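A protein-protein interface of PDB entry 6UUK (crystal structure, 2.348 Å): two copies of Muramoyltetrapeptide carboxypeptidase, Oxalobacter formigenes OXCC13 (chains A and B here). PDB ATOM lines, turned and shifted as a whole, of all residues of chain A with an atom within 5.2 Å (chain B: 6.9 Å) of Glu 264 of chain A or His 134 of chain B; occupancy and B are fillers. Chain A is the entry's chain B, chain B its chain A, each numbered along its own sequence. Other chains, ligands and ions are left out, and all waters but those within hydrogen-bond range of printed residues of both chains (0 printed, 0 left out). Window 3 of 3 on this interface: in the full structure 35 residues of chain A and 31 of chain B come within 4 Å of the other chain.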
ATOM      1  N   LEU A 259       5.029  23.972  18.223  1.00  0.00           N
ATOM      2  CA  LEU A 259       4.141  23.315  19.176  1.00  0.00           C
ATOM      3  C   LEU A 259       3.896  21.861  18.797  1.00  0.00           C
ATOM      4  O   LEU A 259       3.670  21.023  19.677  1.00  0.00           O
ATOM      5  CB  LEU A 259       2.816  24.072  19.276  1.00  0.00           C
ATOM      6  CG  LEU A 259       2.847  25.404  20.029  1.00  0.00           C
ATOM      7  CD1 LEU A 259       1.493  26.090  19.961  1.00  0.00           C
ATOM      8  CD2 LEU A 259       3.275  25.197  21.473  1.00  0.00           C
ATOM      9  N   LEU A 260       3.933  21.543  17.501  1.00  0.00           N
ATOM     10  CA  LEU A 260       3.802  20.153  17.082  1.00  0.00           C
ATOM     11  C   LEU A 260       5.046  19.345  17.425  1.00  0.00           C
ATOM     12  O   LEU A 260       4.944  18.146  17.709  1.00  0.00           O
ATOM     13  CB  LEU A 260       3.513  20.072  15.583  1.00  0.00           C
ATOM     14  CG  LEU A 260       2.072  20.363  15.156  1.00  0.00           C
ATOM     15  CD1 LEU A 260       1.917  20.216  13.651  1.00  0.00           C
ATOM     16  CD2 LEU A 260       1.103  19.448  15.890  1.00  0.00           C
ATOM     17  N   GLN A 261       6.224  19.976  17.401  1.00  0.00           N
ATOM     18  CA  GLN A 261       7.436  19.277  17.816  1.00  0.00           C
ATOM     19  C   GLN A 261       7.376  18.920  19.294  1.00  0.00           C
ATOM     20  O   GLN A 261       7.759  17.813  19.691  1.00  0.00           O
ATOM     21  CB  GLN A 261       8.669  20.129  17.518  1.00  0.00           C
ATOM     22  CG  GLN A 261       9.980  19.461  17.903  1.00  0.00           C
ATOM     23  CD  GLN A 261      11.192  20.276  17.501  1.00  0.00           C
ATOM     24  OE1 GLN A 261      11.088  21.471  17.227  1.00  0.00           O
ATOM     25  NE2 GLN A 261      12.352  19.631  17.459  1.00  0.00           N
ATOM     26  N   LEU A 262       6.894  19.845  20.126  1.00  0.00           N
ATOM     27  CA  LEU A 262       6.695  19.540  21.538  1.00  0.00           C
ATOM     28  C   LEU A 262       5.580  18.527  21.757  1.00  0.00           C
ATOM     29  O   LEU A 262       5.563  17.861  22.796  1.00  0.00           O
ATOM     30  CB  LEU A 262       6.393  20.819  22.318  1.00  0.00           C
ATOM     31  CG  LEU A 262       7.425  21.940  22.186  1.00  0.00           C
ATOM     32  CD1 LEU A 262       7.023  23.149  23.016  1.00  0.00           C
ATOM     33  CD2 LEU A 262       8.810  21.448  22.580  1.00  0.00           C
ATOM     34  N   ASP A 263       4.651  18.397  20.808  1.00  0.00           N
ATOM     35  CA  ASP A 263       3.597  17.400  20.944  1.00  0.00           C
ATOM     36  C   ASP A 263       4.046  16.037  20.427  1.00  0.00           C
ATOM     37  O   ASP A 263       3.783  15.013  21.067  1.00  0.00           O
ATOM     38  CB  ASP A 263       2.336  17.869  20.220  1.00  0.00           C
ATOM     39  CG  ASP A 263       1.216  16.851  20.283  1.00  0.00           C
ATOM     40  OD1 ASP A 263       0.688  16.603  21.391  1.00  0.00           O
ATOM     41  OD2 ASP A 263       0.860  16.297  19.221  1.00  0.00           O
ATOM     42  N   GLU A 264       4.729  16.006  19.281  1.00  0.00           N
ATOM     43  CA  GLU A 264       5.225  14.740  18.748  1.00  0.00           C
ATOM     44  C   GLU A 264       6.320  14.148  19.629  1.00  0.00           C
ATOM     45  O   GLU A 264       6.415  12.921  19.758  1.00  0.00           O
ATOM     46  CB  GLU A 264       5.736  14.931  17.319  1.00  0.00           C
ATOM     47  CG  GLU A 264       4.641  15.255  16.314  1.00  0.00           C
ATOM     48  CD  GLU A 264       3.684  14.098  16.101  1.00  0.00           C
ATOM     49  OE1 GLU A 264       4.096  12.938  16.308  1.00  0.00           O
ATOM     50  OE2 GLU A 264       2.519  14.348  15.729  1.00  0.00           O
ATOM     51  N   SER A 265       7.150  14.994  20.243  1.00  0.00           N
ATOM     52  CA  SER A 265       8.168  14.504  21.166  1.00  0.00           C
ATOM     53  C   SER A 265       7.576  13.980  22.467  1.00  0.00           C
ATOM     54  O   SER A 265       8.306  13.374  23.260  1.00  0.00           O
ATOM     55  CB  SER A 265       9.182  15.608  21.472  1.00  0.00           C
ATOM     56  OG  SER A 265       9.829  16.052  20.292  1.00  0.00           O
ATOM     57  N   GLY A 266       6.287  14.200  22.708  1.00  0.00           N
ATOM     58  CA  GLY A 266       5.627  13.700  23.895  1.00  0.00           C
ATOM     59  C   GLY A 266       5.656  14.622  25.092  1.00  0.00           C
ATOM     60  O   GLY A 266       5.316  14.182  26.197  1.00  0.00           O
ATOM     61  N   ARG A 303      -6.345  19.226  18.443  1.00  0.00           N
ATOM     62  CA  ARG A 303      -5.292  18.218  18.404  1.00  0.00           C
ATOM     63  C   ARG A 303      -4.829  17.840  19.807  1.00  0.00           C
ATOM     64  O   ARG A 303      -4.729  16.653  20.136  1.00  0.00           O
ATOM     65  CB  ARG A 303      -4.114  18.725  17.569  1.00  0.00           C
ATOM     66  CG  ARG A 303      -2.795  18.009  17.843  1.00  0.00           C
ATOM     67  CD  ARG A 303      -2.834  16.552  17.404  1.00  0.00           C
ATOM     68  NE  ARG A 303      -2.694  16.409  15.958  1.00  0.00           N
ATOM     69  CZ  ARG A 303      -1.536  16.199  15.339  1.00  0.00           C
ATOM     70  NH1 ARG A 303      -0.415  16.109  16.041  1.00  0.00           N
ATOM     71  NH2 ARG A 303      -1.499  16.080  14.019  1.00  0.00           N
ATOM     72  N   SER B 105      -4.567  14.198   3.488  1.00  0.00           N
ATOM     73  CA  SER B 105      -4.067  12.873   3.837  1.00  0.00           C
ATOM     74  C   SER B 105      -4.580  11.814   2.869  1.00  0.00           C
ATOM     75  O   SER B 105      -3.843  10.891   2.508  1.00  0.00           O
ATOM     76  CB  SER B 105      -4.470  12.515   5.267  1.00  0.00           C
ATOM     77  OG  SER B 105      -3.918  13.426   6.202  1.00  0.00           O
ATOM     78  N   THR B 130       3.498  18.057   8.420  1.00  0.00           N
ATOM     79  CA  THR B 130       3.574  17.480   9.757  1.00  0.00           C
ATOM     80  C   THR B 130       2.185  17.156  10.291  1.00  0.00           C
ATOM     81  O   THR B 130       2.025  16.212  11.071  1.00  0.00           O
ATOM     82  CB  THR B 130       4.308  18.431  10.704  1.00  0.00           C
ATOM     83  OG1 THR B 130       5.558  18.819  10.117  1.00  0.00           O
ATOM     84  CG2 THR B 130       4.581  17.754  12.040  1.00  0.00           C
ATOM     85  N   ARG B 131       1.174  17.923   9.873  1.00  0.00           N
ATOM     86  CA  ARG B 131      -0.205  17.568  10.187  1.00  0.00           C
ATOM     87  C   ARG B 131      -0.576  16.211   9.608  1.00  0.00           C
ATOM     88  O   ARG B 131      -1.463  15.531  10.136  1.00  0.00           O
ATOM     89  CB  ARG B 131      -1.161  18.636   9.653  1.00  0.00           C
ATOM     90  CG  ARG B 131      -1.036  20.004  10.300  1.00  0.00           C
ATOM     91  CD  ARG B 131      -2.114  20.933   9.763  1.00  0.00           C
ATOM     92  NE  ARG B 131      -2.233  22.169  10.529  1.00  0.00           N
ATOM     93  CZ  ARG B 131      -3.208  23.056  10.360  1.00  0.00           C
ATOM     94  NH1 ARG B 131      -4.151  22.839   9.453  1.00  0.00           N
ATOM     95  NH2 ARG B 131      -3.245  24.157  11.098  1.00  0.00           N
ATOM     96  N   LEU B 132       0.088  15.802   8.532  1.00  0.00           N
ATOM     97  CA  LEU B 132      -0.241  14.563   7.828  1.00  0.00           C
ATOM     98  C   LEU B 132       0.761  13.465   8.178  1.00  0.00           C
ATOM     99  O   LEU B 132       1.514  12.975   7.336  1.00  0.00           O
ATOM    100  CB  LEU B 132      -0.283  14.810   6.322  1.00  0.00           C
ATOM    101  CG  LEU B 132      -0.979  16.071   5.808  1.00  0.00           C
ATOM    102  CD1 LEU B 132      -1.061  16.033   4.290  1.00  0.00           C
ATOM    103  CD2 LEU B 132      -2.360  16.239   6.419  1.00  0.00           C
ATOM    104  N   LEU B 133       0.761  13.076   9.447  1.00  0.00           N
ATOM    105  CA  LEU B 133       1.640  12.019   9.933  1.00  0.00           C
ATOM    106  C   LEU B 133       0.896  10.894  10.632  1.00  0.00           C
ATOM    107  O   LEU B 133       1.247   9.725  10.456  1.00  0.00           O
ATOM    108  CB  LEU B 133       2.697  12.602  10.883  1.00  0.00           C
ATOM    109  CG  LEU B 133       3.815  13.422  10.235  1.00  0.00           C
ATOM    110  CD1 LEU B 133       4.784  13.938  11.287  1.00  0.00           C
ATOM    111  CD2 LEU B 133       4.547  12.594   9.190  1.00  0.00           C
ATOM    112  N   HIS B 134      -0.128  11.218  11.423  1.00  0.00           N
ATOM    113  CA  HIS B 134      -0.922  10.210  12.112  1.00  0.00           C
ATOM    114  C   HIS B 134      -2.032   9.639  11.242  1.00  0.00           C
ATOM    115  O   HIS B 134      -2.375   8.459  11.384  1.00  0.00           O
ATOM    116  CB  HIS B 134      -1.525  10.800  13.390  1.00  0.00           C
ATOM    117  CG  HIS B 134      -0.502  11.262  14.379  1.00  0.00           C
ATOM    118  ND1 HIS B 134       0.790  10.782  14.392  1.00  0.00           N
ATOM    119  CD2 HIS B 134      -0.577  12.166  15.384  1.00  0.00           C
ATOM    120  CE1 HIS B 134       1.464  11.367  15.366  1.00  0.00           C
ATOM    121  NE2 HIS B 134       0.658  12.211  15.983  1.00  0.00           N
ATOM    122  N   ASP B 135      -2.604  10.446  10.348  1.00  0.00           N
ATOM    123  CA  ASP B 135      -3.631   9.954   9.440  1.00  0.00           C
ATOM    124  C   ASP B 135      -3.059   9.145   8.284  1.00  0.00           C
ATOM    125  O   ASP B 135      -3.832   8.615   7.479  1.00  0.00           O
ATOM    126  CB  ASP B 135      -4.449  11.120   8.881  1.00  0.00           C
ATOM    127  CG  ASP B 135      -5.144  11.920   9.965  1.00  0.00           C
ATOM    128  OD1 ASP B 135      -5.503  11.331  11.007  1.00  0.00           O
ATOM    129  OD2 ASP B 135      -5.332  13.140   9.773  1.00  0.00           O
ATOM    130  N   LEU B 136      -1.738   9.037   8.183  1.00  0.00           N
ATOM    131  CA  LEU B 136      -1.084   8.324   7.097  1.00  0.00           C
ATOM    132  C   LEU B 136      -0.475   7.028   7.613  1.00  0.00           C
ATOM    133  O   LEU B 136      -0.125   6.909   8.790  1.00  0.00           O
ATOM    134  CB  LEU B 136       0.005   9.182   6.442  1.00  0.00           C
ATOM    135  CG  LEU B 136      -0.416  10.277   5.456  1.00  0.00           C
ATOM    136  CD1 LEU B 136      -1.202  11.381   6.138  1.00  0.00           C
ATOM    137  CD2 LEU B 136       0.799  10.850   4.746  1.00  0.00           C
ATOM    138  N   ASP B 137      -0.354   6.054   6.716  1.00  0.00           N
ATOM    139  CA  ASP B 137       0.229   4.752   7.027  1.00  0.00           C
ATOM    140  C   ASP B 137       1.517   4.625   6.217  1.00  0.00           C
ATOM    141  O   ASP B 137       1.505   4.206   5.059  1.00  0.00           O
ATOM    142  CB  ASP B 137      -0.752   3.622   6.715  1.00  0.00           C
ATOM    143  CG  ASP B 137      -0.302   2.286   7.277  1.00  0.00           C
ATOM    144  OD1 ASP B 137       0.753   2.242   7.944  1.00  0.00           O
ATOM    145  OD2 ASP B 137      -1.007   1.280   7.054  1.00  0.00           O
ATOM    146  N   PHE B 138       2.639   4.995   6.841  1.00  0.00           N
ATOM    147  CA  PHE B 138       3.927   4.922   6.161  1.00  0.00           C
ATOM    148  C   PHE B 138       4.394   3.488   5.953  1.00  0.00           C
ATOM    149  O   PHE B 138       5.292   3.256   5.137  1.00  0.00           O
ATOM    150  CB  PHE B 138       4.978   5.713   6.941  1.00  0.00           C
ATOM    151  CG  PHE B 138       4.821   7.201   6.826  1.00  0.00           C
ATOM    152  CD1 PHE B 138       4.021   7.900   7.713  1.00  0.00           C
ATOM    153  CD2 PHE B 138       5.468   7.902   5.821  1.00  0.00           C
ATOM    154  CE1 PHE B 138       3.873   9.271   7.605  1.00  0.00           C
ATOM    155  CE2 PHE B 138       5.325   9.270   5.707  1.00  0.00           C
ATOM    156  CZ  PHE B 138       4.525   9.956   6.600  1.00  0.00           C
ATOM    157  N   HIS B 228      13.104  20.337  13.416  1.00  0.00           N
ATOM    158  CA  HIS B 228      11.736  20.101  13.857  1.00  0.00           C
ATOM    159  C   HIS B 228      11.475  18.628  14.152  1.00  0.00           C
ATOM    160  O   HIS B 228      10.567  18.315  14.928  1.00  0.00           O
ATOM    161  CB  HIS B 228      10.761  20.623  12.798  1.00  0.00           C
ATOM    162  CG  HIS B 228       9.334  20.250  13.046  1.00  0.00           C
ATOM    163  ND1 HIS B 228       8.676  20.554  14.219  1.00  0.00           N
ATOM    164  CD2 HIS B 228       8.434  19.600  12.270  1.00  0.00           C
ATOM    165  CE1 HIS B 228       7.436  20.103  14.156  1.00  0.00           C
ATOM    166  NE2 HIS B 228       7.263  19.521  12.983  1.00  0.00           N
ATOM    167  N   MET B 229      12.255  17.724  13.568  1.00  0.00           N
ATOM    168  CA  MET B 229      12.072  16.291  13.777  1.00  0.00           C
ATOM    169  C   MET B 229      12.769  15.799  15.045  1.00  0.00           C
ATOM    170  O   MET B 229      12.545  14.669  15.483  1.00  0.00           O
ATOM    171  CB  MET B 229      12.590  15.504  12.570  1.00  0.00           C
ATOM    172  CG  MET B 229      11.847  15.763  11.269  1.00  0.00           C
ATOM    173  SD  MET B 229      10.468  14.442  10.873  1.00  0.00           S
ATOM    174  CE  MET B 229       9.144  14.944  12.214  1.00  0.00           C
ATOM    175  N   GLY B 231      13.710  14.775  18.583  1.00  0.00           N
ATOM    176  CA  GLY B 231      12.924  14.331  19.713  1.00  0.00           C
ATOM    177  C   GLY B 231      11.638  13.616  19.361  1.00  0.00           C
ATOM    178  O   GLY B 231      10.992  13.060  20.260  1.00  0.00           O
ATOM    179  N   THR B 232      11.247  13.607  18.086  1.00  0.00           N
ATOM    180  CA  THR B 232      10.015  12.999  17.614  1.00  0.00           C
ATOM    181  C   THR B 232      10.268  11.580  17.117  1.00  0.00           C
ATOM    182  O   THR B 232      11.370  11.264  16.658  1.00  0.00           O
ATOM    183  CB  THR B 232       9.404  13.831  16.482  1.00  0.00           C
ATOM    184  OG1 THR B 232      10.219  13.717  15.309  1.00  0.00           O
ATOM    185  CG2 THR B 232       9.321  15.293  16.887  1.00  0.00           C
ATOM    186  N   PRO B 233       9.267  10.697  17.200  1.00  0.00           N
ATOM    187  CA  PRO B 233       9.449   9.327  16.694  1.00  0.00           C
ATOM    188  C   PRO B 233       9.612   9.244  15.186  1.00  0.00           C
ATOM    189  O   PRO B 233       9.987   8.178  14.683  1.00  0.00           O
ATOM    190  CB  PRO B 233       8.168   8.609  17.147  1.00  0.00           C
ATOM    191  CG  PRO B 233       7.610   9.460  18.244  1.00  0.00           C
ATOM    192  CD  PRO B 233       7.973  10.864  17.882  1.00  0.00           C
ATOM    193  N   TRP B 234       9.345  10.323  14.451  1.00  0.00           N
ATOM    194  CA  TRP B 234       9.453  10.310  12.998  1.00  0.00           C
ATOM    195  C   TRP B 234      10.873  10.554  12.504  1.00  0.00           C
ATOM    196  O   TRP B 234      11.089  10.588  11.288  1.00  0.00           O
ATOM    197  CB  TRP B 234       8.507  11.353  12.398  1.00  0.00           C
ATOM    198  CG  TRP B 234       7.122  11.290  12.963  1.00  0.00           C
ATOM    199  CD1 TRP B 234       6.590  12.101  13.923  1.00  0.00           C
ATOM    200  CD2 TRP B 234       6.092  10.357  12.611  1.00  0.00           C
ATOM    201  NE1 TRP B 234       5.291  11.734  14.187  1.00  0.00           N
ATOM    202  CE2 TRP B 234       4.963  10.666  13.394  1.00  0.00           C
ATOM    203  CE3 TRP B 234       6.015   9.294  11.708  1.00  0.00           C
ATOM    204  CZ2 TRP B 234       3.772   9.951  13.301  1.00  0.00           C
ATOM    205  CZ3 TRP B 234       4.833   8.584  11.616  1.00  0.00           C
ATOM    206  CH2 TRP B 234       3.726   8.915  12.409  1.00  0.00           C
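No position is printed for both chains.
The side-chain hydroxyl (OG1) of Thr 130 of chain B lies close to a ring nitrogen (NE2) of His 228 of chain B, 3.4 Å away. The backbone carbonyl oxygen of Met 229 of chain B sits at hydrogen-bond distance from the side-chain hydroxyl of Thr 232 of chain B, 2.5 Å away. The side-chain hydroxyl (OG) of Ser 265 of chain A is in hydrogen-bond range of the backbone carbonyl oxygen (O) of Gln 261 of chain A (2.8 Å). The guanidinium group (NH1) of Arg 303 of chain A lies within salt-bridge range of the side-chain carboxylate (OE2) of Glu 264 of chain A, 3.4 Å away. The side-chain carboxylate (OD2) of Asp 263 of chain A lies within salt-bridge range of the guanidinium group (NH1) of Arg 303 of chain A (3.4 Å).
Leu 262 of chain A touches none of the printed residues of chain B. Printed residues of chain A within 4 Å of His 134 of chain B: Glu 264. Met 229 of chain B touches none of the printed residues of chain A. Printed residues of chain A within 4 Å of Thr 232 of chain B: Glu 264 (3.6 Å) and Ser 265 (3.5 Å). Printed residues of chain A within 4 Å of Pro 233 of chain B: Glu 264. Printed residues of chain A within 4 Å of Trp 234 of chain B: Glu 264. The nearest printed residue of chain A that does not touch His 134 of chain B is Arg 303 of chain A (4.001 Å). The nearest printed residue of chain B that does not touch Arg 303 of chain A is His 134 of chain B (4.001 Å).
Hydrophobic or aromatic side chains of chain B within 4 Å of the printed part of chain A: His 134, His 228, Pro 233 and Trp 234. Among the printed residues, 9 pairs touch across the chains. Among the printed residues, no Asp or Glu carboxylate lies within 4 Å of a Lys or Arg side-chain nitrogen of the other chain.
NE2 of His 134 of chain B lies within hydrogen-bond range of OE2 of Glu 264 of chain A. The side-chain carboxylate (OE1) of Glu 264 of chain A is in hydrogen-bond range of the indole nitrogen (NE1) of Trp 234 of chain B (2.7 Å). O of His 228 of chain B sits close to NE2 of Gln 261 of chain A. O of Gly 231 of chain B lies close to OG of Ser 265 of chain A, 3.2 Å away.
Leu 260 of chain A touches Thr 130 of chain B. CG2 of Thr 232 of chain B touches CB of Glu 264 of chain A (3.6 Å). O of Glu 264 of chain A touches CD of Pro 233 of chain B, at 3.2 Å. OG of Ser 265 of chain A touches CG2 of Thr 232 of chain B, 3.5 Å away. Arg 303 of chain A touches Arg 131 of chain B.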
